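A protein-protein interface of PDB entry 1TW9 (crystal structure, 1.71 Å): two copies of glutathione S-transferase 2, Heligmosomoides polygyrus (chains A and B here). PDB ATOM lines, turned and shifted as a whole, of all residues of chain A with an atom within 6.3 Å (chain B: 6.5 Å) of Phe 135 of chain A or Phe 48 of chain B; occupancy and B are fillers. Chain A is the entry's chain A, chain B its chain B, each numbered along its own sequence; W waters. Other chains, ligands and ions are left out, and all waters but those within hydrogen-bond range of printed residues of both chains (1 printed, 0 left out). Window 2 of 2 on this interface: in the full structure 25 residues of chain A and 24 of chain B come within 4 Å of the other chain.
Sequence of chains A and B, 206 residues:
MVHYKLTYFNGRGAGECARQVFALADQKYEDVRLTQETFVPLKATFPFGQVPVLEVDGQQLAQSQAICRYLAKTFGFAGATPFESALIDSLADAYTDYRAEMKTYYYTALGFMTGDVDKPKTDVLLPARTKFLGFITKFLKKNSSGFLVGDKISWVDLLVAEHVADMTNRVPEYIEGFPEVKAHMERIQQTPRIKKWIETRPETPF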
ATOM      1  N   LEU A  87     -16.430 -33.742  -2.825  1.00  0.00           N
ATOM      2  CA  LEU A  87     -15.160 -33.134  -3.290  1.00  0.00           C
ATOM      3  C   LEU A  87     -14.982 -33.271  -4.774  1.00  0.00           C
ATOM      4  O   LEU A  87     -14.538 -32.333  -5.441  1.00  0.00           O
ATOM      5  CB  LEU A  87     -14.006 -33.782  -2.543  1.00  0.00           C
ATOM      6  CG  LEU A  87     -13.910 -33.373  -1.064  1.00  0.00           C
ATOM      7  CD1 LEU A  87     -12.795 -34.205  -0.392  1.00  0.00           C
ATOM      8  CD2 LEU A  87     -13.661 -31.877  -0.791  1.00  0.00           C
ATOM      9  N   SER A  90     -17.084 -30.851  -6.371  1.00  0.00           N
ATOM     10  CA  SER A  90     -16.557 -29.495  -6.216  1.00  0.00           C
ATOM     11  C   SER A  90     -15.478 -29.244  -7.292  1.00  0.00           C
ATOM     12  O   SER A  90     -15.427 -28.149  -7.859  1.00  0.00           O
ATOM     13  CB  SER A  90     -16.001 -29.223  -4.796  1.00  0.00           C
ATOM     14  OG  SER A  90     -14.766 -29.860  -4.613  1.00  0.00           O
ATOM     15  N   LEU A  91     -14.653 -30.260  -7.598  1.00  0.00           N
ATOM     16  CA  LEU A  91     -13.600 -30.097  -8.613  1.00  0.00           C
ATOM     17  C   LEU A  91     -14.221 -29.942 -10.023  1.00  0.00           C
ATOM     18  O   LEU A  91     -13.713 -29.207 -10.851  1.00  0.00           O
ATOM     19  CB  LEU A  91     -12.625 -31.283  -8.553  1.00  0.00           C
ATOM     20  CG  LEU A  91     -11.679 -31.110  -7.345  1.00  0.00           C
ATOM     21  CD1 LEU A  91     -11.220 -32.477  -6.983  1.00  0.00           C
ATOM     22  CD2 LEU A  91     -10.563 -30.199  -7.776  1.00  0.00           C
ATOM     23  N   ALA A  94     -15.546 -26.471 -10.224  1.00  0.00           N
ATOM     24  CA  ALA A  94     -14.395 -25.567 -10.473  1.00  0.00           C
ATOM     25  C   ALA A  94     -13.959 -25.650 -11.912  1.00  0.00           C
ATOM     26  O   ALA A  94     -13.588 -24.647 -12.515  1.00  0.00           O
ATOM     27  CB  ALA A  94     -13.249 -25.897  -9.559  1.00  0.00           C
ATOM     28  N   THR A 130      -3.349 -21.027 -15.308  1.00  0.00           N
ATOM     29  CA  THR A 130      -2.533 -20.891 -14.106  1.00  0.00           C
ATOM     30  C   THR A 130      -3.358 -20.960 -12.797  1.00  0.00           C
ATOM     31  O   THR A 130      -2.976 -21.650 -11.829  1.00  0.00           O
ATOM     32  CB  THR A 130      -1.776 -19.565 -14.168  1.00  0.00           C
ATOM     33  OG1 THR A 130      -0.857 -19.582 -15.277  1.00  0.00           O
ATOM     34  CG2 THR A 130      -0.861 -19.254 -12.911  1.00  0.00           C
ATOM     35  N   LYS A 131      -4.479 -20.241 -12.768  1.00  0.00           N
ATOM     36  CA  LYS A 131      -5.357 -20.250 -11.633  1.00  0.00           C
ATOM     37  C   LYS A 131      -5.967 -21.637 -11.399  1.00  0.00           C
ATOM     38  O   LYS A 131      -5.812 -22.203 -10.313  1.00  0.00           O
ATOM     39  CB  LYS A 131      -6.471 -19.246 -11.834  1.00  0.00           C
ATOM     40  CG  LYS A 131      -7.350 -19.100 -10.593  1.00  0.00           C
ATOM     41  CD  LYS A 131      -8.148 -17.784 -10.617  1.00  0.00           C
ATOM     42  CE  LYS A 131      -9.059 -17.678 -11.849  1.00  0.00           C
ATOM     43  NZ  LYS A 131     -10.104 -16.563 -11.825  1.00  0.00           N
ATOM     44  N   PHE A 132      -6.598 -22.201 -12.421  1.00  0.00           N
ATOM     45  CA  PHE A 132      -7.204 -23.517 -12.314  1.00  0.00           C
ATOM     46  C   PHE A 132      -6.233 -24.670 -12.049  1.00  0.00           C
ATOM     47  O   PHE A 132      -6.463 -25.495 -11.163  1.00  0.00           O
ATOM     48  CB  PHE A 132      -7.977 -23.855 -13.582  1.00  0.00           C
ATOM     49  CG  PHE A 132      -8.637 -25.176 -13.546  1.00  0.00           C
ATOM     50  CD1 PHE A 132      -8.290 -26.133 -14.464  1.00  0.00           C
ATOM     51  CD2 PHE A 132      -9.668 -25.414 -12.635  1.00  0.00           C
ATOM     52  CE1 PHE A 132      -8.959 -27.363 -14.458  1.00  0.00           C
ATOM     53  CE2 PHE A 132     -10.315 -26.643 -12.605  1.00  0.00           C
ATOM     54  CZ  PHE A 132      -9.908 -27.625 -13.498  1.00  0.00           C
ATOM     55  N   LEU A 133      -5.119 -24.673 -12.756  1.00  0.00           N
ATOM     56  CA  LEU A 133      -4.126 -25.753 -12.533  1.00  0.00           C
ATOM     57  C   LEU A 133      -3.462 -25.611 -11.185  1.00  0.00           C
ATOM     58  O   LEU A 133      -3.012 -26.580 -10.610  1.00  0.00           O
ATOM     59  CB  LEU A 133      -3.167 -25.910 -13.695  1.00  0.00           C
ATOM     60  CG  LEU A 133      -3.783 -26.388 -15.061  1.00  0.00           C
ATOM     61  CD1 LEU A 133      -2.657 -26.730 -15.998  1.00  0.00           C
ATOM     62  CD2 LEU A 133      -4.785 -27.539 -15.010  1.00  0.00           C
ATOM     63  N   GLY A 134      -3.374 -24.399 -10.681  1.00  0.00           N
ATOM     64  CA  GLY A 134      -2.848 -24.219  -9.344  1.00  0.00           C
ATOM     65  C   GLY A 134      -3.771 -24.919  -8.363  1.00  0.00           C
ATOM     66  O   GLY A 134      -3.295 -25.614  -7.428  1.00  0.00           O
ATOM     67  N   PHE A 135      -5.083 -24.712  -8.502  1.00  0.00           N
ATOM     68  CA  PHE A 135      -6.054 -25.381  -7.589  1.00  0.00           C
ATOM     69  C   PHE A 135      -5.982 -26.904  -7.707  1.00  0.00           C
ATOM     70  O   PHE A 135      -5.914 -27.616  -6.673  1.00  0.00           O
ATOM     71  CB  PHE A 135      -7.502 -24.944  -7.868  1.00  0.00           C
ATOM     72  CG  PHE A 135      -7.766 -23.472  -7.622  1.00  0.00           C
ATOM     73  CD1 PHE A 135      -8.568 -22.751  -8.500  1.00  0.00           C
ATOM     74  CD2 PHE A 135      -7.232 -22.812  -6.538  1.00  0.00           C
ATOM     75  CE1 PHE A 135      -8.829 -21.410  -8.283  1.00  0.00           C
ATOM     76  CE2 PHE A 135      -7.496 -21.497  -6.318  1.00  0.00           C
ATOM     77  CZ  PHE A 135      -8.295 -20.780  -7.209  1.00  0.00           C
ATOM     78  N   ILE A 136      -5.963 -27.392  -8.924  1.00  0.00           N
ATOM     79  CA  ILE A 136      -5.837 -28.842  -9.211  1.00  0.00           C
ATOM     80  C   ILE A 136      -4.579 -29.433  -8.599  1.00  0.00           C
ATOM     81  O   ILE A 136      -4.613 -30.493  -7.970  1.00  0.00           O
ATOM     82  CB  ILE A 136      -5.861 -29.142 -10.776  1.00  0.00           C
ATOM     83  CG1 ILE A 136      -7.193 -28.819 -11.390  1.00  0.00           C
ATOM     84  CG2 ILE A 136      -5.501 -30.668 -11.070  1.00  0.00           C
ATOM     85  CD1 ILE A 136      -8.355 -29.372 -10.671  1.00  0.00           C
ATOM     86  N   THR A 137      -3.450 -28.746  -8.762  1.00  0.00           N
ATOM     87  CA  THR A 137      -2.159 -29.175  -8.217  1.00  0.00           C
ATOM     88  C   THR A 137      -2.171 -29.333  -6.686  1.00  0.00           C
ATOM     89  O   THR A 137      -1.633 -30.309  -6.123  1.00  0.00           O
ATOM     90  CB  THR A 137      -1.096 -28.195  -8.644  1.00  0.00           C
ATOM     91  OG1 THR A 137      -0.970 -28.261 -10.083  1.00  0.00           O
ATOM     92  CG2 THR A 137       0.262 -28.652  -8.121  1.00  0.00           C
ATOM     93  N   LYS A 138      -2.846 -28.408  -6.018  1.00  0.00           N
ATOM     94  CA  LYS A 138      -3.025 -28.460  -4.584  1.00  0.00           C
ATOM     95  C   LYS A 138      -3.775 -29.736  -4.170  1.00  0.00           C
ATOM     96  O   LYS A 138      -3.349 -30.382  -3.250  1.00  0.00           O
ATOM     97  CB  LYS A 138      -3.722 -27.183  -4.145  1.00  0.00           C
ATOM     98  CG  LYS A 138      -4.238 -27.137  -2.830  1.00  0.00           C
ATOM     99  CD  LYS A 138      -4.809 -25.710  -2.559  1.00  0.00           C
ATOM    100  CE  LYS A 138      -6.288 -25.512  -3.081  1.00  0.00           C
ATOM    101  NZ  LYS A 138      -6.657 -24.097  -2.643  1.00  0.00           N
ATOM    102  N   PHE A 139      -4.825 -30.109  -4.900  1.00  0.00           N
ATOM    103  CA  PHE A 139      -5.510 -31.359  -4.648  1.00  0.00           C
ATOM    104  C   PHE A 139      -4.606 -32.594  -4.912  1.00  0.00           C
ATOM    105  O   PHE A 139      -4.546 -33.522  -4.090  1.00  0.00           O
ATOM    106  CB  PHE A 139      -6.812 -31.403  -5.458  1.00  0.00           C
ATOM    107  CG  PHE A 139      -7.939 -30.687  -4.793  1.00  0.00           C
ATOM    108  CD1 PHE A 139      -8.056 -29.331  -4.839  1.00  0.00           C
ATOM    109  CD2 PHE A 139      -8.933 -31.409  -4.102  1.00  0.00           C
ATOM    110  CE1 PHE A 139      -9.121 -28.658  -4.262  1.00  0.00           C
ATOM    111  CE2 PHE A 139      -9.987 -30.725  -3.481  1.00  0.00           C
ATOM    112  CZ  PHE A 139     -10.088 -29.364  -3.542  1.00  0.00           C
ATOM    113  N   LEU A 140      -3.904 -32.598  -6.048  1.00  0.00           N
ATOM    114  CA  LEU A 140      -2.976 -33.691  -6.342  1.00  0.00           C
ATOM    115  C   LEU A 140      -1.918 -33.820  -5.281  1.00  0.00           C
ATOM    116  O   LEU A 140      -1.578 -34.933  -4.791  1.00  0.00           O
ATOM    117  CB  LEU A 140      -2.310 -33.480  -7.684  1.00  0.00           C
ATOM    118  CG  LEU A 140      -3.320 -33.498  -8.804  1.00  0.00           C
ATOM    119  CD1 LEU A 140      -2.814 -32.994 -10.169  1.00  0.00           C
ATOM    120  CD2 LEU A 140      -3.874 -34.909  -9.013  1.00  0.00           C
ATOM    121  N   LYS B  43      -9.280 -14.910   0.599  1.00  0.00           N
ATOM    122  CA  LYS B  43      -9.457 -15.756  -0.570  1.00  0.00           C
ATOM    123  C   LYS B  43      -8.594 -16.997  -0.556  1.00  0.00           C
ATOM    124  O   LYS B  43      -9.065 -18.064  -0.893  1.00  0.00           O
ATOM    125  CB  LYS B  43      -9.167 -15.013  -1.870  1.00  0.00           C
ATOM    126  CG  LYS B  43     -10.311 -14.224  -2.364  1.00  0.00           C
ATOM    127  CD  LYS B  43      -9.907 -13.376  -3.574  1.00  0.00           C
ATOM    128  CE  LYS B  43      -9.713 -14.262  -4.788  1.00  0.00           C
ATOM    129  NZ  LYS B  43     -11.059 -14.619  -5.313  1.00  0.00           N
ATOM    130  N   PHE B  46      -9.581 -20.582   0.867  1.00  0.00           N
ATOM    131  CA  PHE B  46     -10.702 -21.334   0.359  1.00  0.00           C
ATOM    132  C   PHE B  46     -10.217 -22.168  -0.809  1.00  0.00           C
ATOM    133  O   PHE B  46      -9.312 -21.710  -1.547  1.00  0.00           O
ATOM    134  CB  PHE B  46     -11.855 -20.433  -0.116  1.00  0.00           C
ATOM    135  CG  PHE B  46     -12.344 -19.479   0.937  1.00  0.00           C
ATOM    136  CD1 PHE B  46     -12.398 -18.118   0.686  1.00  0.00           C
ATOM    137  CD2 PHE B  46     -12.760 -19.948   2.170  1.00  0.00           C
ATOM    138  CE1 PHE B  46     -12.842 -17.218   1.696  1.00  0.00           C
ATOM    139  CE2 PHE B  46     -13.224 -19.087   3.143  1.00  0.00           C
ATOM    140  CZ  PHE B  46     -13.241 -17.711   2.918  1.00  0.00           C
ATOM    141  N   PRO B  47     -10.809 -23.374  -0.988  1.00  0.00           N
ATOM    142  CA  PRO B  47     -10.276 -24.308  -1.981  1.00  0.00           C
ATOM    143  C   PRO B  47     -10.037 -23.704  -3.386  1.00  0.00           C
ATOM    144  O   PRO B  47      -8.995 -23.995  -3.998  1.00  0.00           O
ATOM    145  CB  PRO B  47     -11.339 -25.400  -2.032  1.00  0.00           C
ATOM    146  CG  PRO B  47     -11.892 -25.484  -0.637  1.00  0.00           C
ATOM    147  CD  PRO B  47     -11.901 -23.981  -0.200  1.00  0.00           C
ATOM    148  N   PHE B  48     -10.997 -22.918  -3.888  1.00  0.00           N
ATOM    149  CA  PHE B  48     -10.902 -22.327  -5.204  1.00  0.00           C
ATOM    150  C   PHE B  48     -10.977 -20.787  -5.163  1.00  0.00           C
ATOM    151  O   PHE B  48     -11.417 -20.118  -6.145  1.00  0.00           O
ATOM    152  CB  PHE B  48     -12.013 -22.849  -6.040  1.00  0.00           C
ATOM    153  CG  PHE B  48     -12.033 -24.320  -6.105  1.00  0.00           C
ATOM    154  CD1 PHE B  48     -13.046 -25.049  -5.450  1.00  0.00           C
ATOM    155  CD2 PHE B  48     -11.044 -24.995  -6.732  1.00  0.00           C
ATOM    156  CE1 PHE B  48     -13.041 -26.432  -5.435  1.00  0.00           C
ATOM    157  CE2 PHE B  48     -11.085 -26.413  -6.735  1.00  0.00           C
ATOM    158  CZ  PHE B  48     -12.047 -27.076  -6.059  1.00  0.00           C
ATOM    159  N   GLY B  49     -10.621 -20.270  -3.992  1.00  0.00           N
ATOM    160  CA  GLY B  49     -10.520 -18.785  -3.777  1.00  0.00           C
ATOM    161  C   GLY B  49     -11.881 -18.089  -3.749  1.00  0.00           C
ATOM    162  O   GLY B  49     -11.977 -16.861  -3.980  1.00  0.00           O
ATOM    163  N   GLN B  50     -12.948 -18.829  -3.445  1.00  0.00           N
ATOM    164  CA  GLN B  50     -14.294 -18.261  -3.558  1.00  0.00           C
ATOM    165  C   GLN B  50     -15.164 -18.799  -2.449  1.00  0.00           C
ATOM    166  O   GLN B  50     -14.815 -19.795  -1.786  1.00  0.00           O
ATOM    167  CB  GLN B  50     -14.948 -18.617  -4.880  1.00  0.00           C
ATOM    168  CG  GLN B  50     -14.254 -18.121  -6.129  1.00  0.00           C
ATOM    169  CD  GLN B  50     -14.707 -18.974  -7.303  1.00  0.00           C
ATOM    170  OE1 GLN B  50     -14.075 -20.008  -7.656  1.00  0.00           O
ATOM    171  NE2 GLN B  50     -15.862 -18.644  -7.819  1.00  0.00           N
ATOM    172  N   VAL B  53     -18.265 -21.767   1.180  1.00  0.00           N
ATOM    173  CA  VAL B  53     -17.510 -22.962   1.544  1.00  0.00           C
ATOM    174  C   VAL B  53     -18.173 -23.506   2.775  1.00  0.00           C
ATOM    175  O   VAL B  53     -18.477 -22.779   3.717  1.00  0.00           O
ATOM    176  CB  VAL B  53     -15.990 -22.624   1.852  1.00  0.00           C
ATOM    177  CG1 VAL B  53     -15.220 -23.915   2.288  1.00  0.00           C
ATOM    178  CG2 VAL B  53     -15.312 -22.054   0.574  1.00  0.00           C
ATOM    179  N   ALA B  62     -16.151 -26.777  -1.073  1.00  0.00           N
ATOM    180  CA  ALA B  62     -16.529 -25.620  -1.811  1.00  0.00           C
ATOM    181  C   ALA B  62     -17.520 -25.942  -2.898  1.00  0.00           C
ATOM    182  O   ALA B  62     -17.774 -27.099  -3.213  1.00  0.00           O
ATOM    183  CB  ALA B  62     -15.273 -24.943  -2.411  1.00  0.00           C
ATOM    184  N   GLN B  63     -18.088 -24.867  -3.459  1.00  0.00           N
ATOM    185  CA  GLN B  63     -18.878 -24.813  -4.708  1.00  0.00           C
ATOM    186  C   GLN B  63     -20.334 -25.041  -4.326  1.00  0.00           C
ATOM    187  O   GLN B  63     -20.718 -26.074  -3.725  1.00  0.00           O
ATOM    188  CB  GLN B  63     -18.412 -25.787  -5.770  1.00  0.00           C
ATOM    189  CG  GLN B  63     -17.005 -25.572  -6.284  1.00  0.00           C
ATOM    190  CD  GLN B  63     -16.847 -24.399  -7.263  1.00  0.00           C
ATOM    191  OE1 GLN B  63     -15.734 -23.826  -7.449  1.00  0.00           O
ATOM    192  NE2 GLN B  63     -17.934 -24.030  -7.884  1.00  0.00           N
HETATM  193  O   HOH W   1     -14.062 -28.316  -2.358  1.00  0.00           O
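Of the 9 printed residues of chain B, 5 touch a printed residue of chain A.
Printed residues of chain B that touch a printed residue of chain A: Phe 46, Pro 47, Phe 48, Ala 62 and Gln 63.
Hydrophobic or aromatic side chains of chain B that line the printed part of chain A: Phe 48.
Along chain B the printed residues that touch a printed residue of chain A span positions 46 to 63.
Among the printed residues, 11 pairs touch across the chains.
Among the printed residues, no Asp or Glu carboxylate lies within 4 Å of a Lys or Arg side-chain nitrogen of the other chain.
The side-chain amino group (NZ) of Lys 138 of chain A lies within hydrogen-bond range of the backbone carbonyl oxygen (O) of Pro 47 of chain B.
O of Phe 48 of chain B lies close to OE1 of Gln 50 of chain B (3.1 Å).
The backbone carbonyl oxygen (O) of Leu 87 of chain A is in hydrogen-bond range of the side-chain hydroxyl (OG) of Ser 90 of chain A, 2.6 Å away.
Leu 87 of chain A touches none of the printed residues of chain B.
Of the printed residues of chain B, Ser 90 of chain A touches Phe 48, Ala 62 and Gln 63.
Of the printed residues of chain B, Leu 91 of chain A touches Phe 48.
Phe 132 of chain A touches none of the printed residues of chain B.
Of the printed residues of chain B, Phe 135 of chain A touches Pro 47 (3.3 Å) and Phe 48 (3.4 Å).
Of the printed residues of chain B, Lys 138 of chain A touches Phe 46 and Pro 47.
Of the printed residues of chain B, Phe 139 of chain A touches Phe 48.
Printed residues of chain A within 4 Å of Phe 46 of chain B: Lys 138.
Phe 48 of chain B touches five residues of chain A.
The nearest residue of chain A that does not touch Phe 48 of chain B is Lys 138 of chain A (4.7 Å).
The nearest printed residue of chain B that does not touch Lys 138 of chain A is Phe 48 of chain B (4.7 Å).
No position is printed for both chains.
Of the 11 pairs that touch across the chains among the printed residues, none has its exchanged pair printed and touching as well.
Water W1 lies within hydrogen-bond range of the side-chain hydroxyl of Ser 90 of chain A (2.8 Å) and the backbone NH of Ala 62 of chain B (2.9 Å).
Among the printed residues, merely in contact across the chains: Ser 90 of chain A with Phe 48 of chain B, Ser 90 of chain A with Ala 62 of chain B, Ser 90 of chain A with Gln 63 of chain B, Leu 91 of chain A with Phe 48 of chain B, Ala 94 of chain A with Phe 48 of chain B, Ala 94 of chain A with Gln 63 of chain B, Phe 135 of chain A with Pro 47 of chain B, Phe 135 of chain A with Phe 48 of chain B, Lys 138 of chain A with Phe 46 of chain B and Phe 139 of chain A with Phe 48 of chain B.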
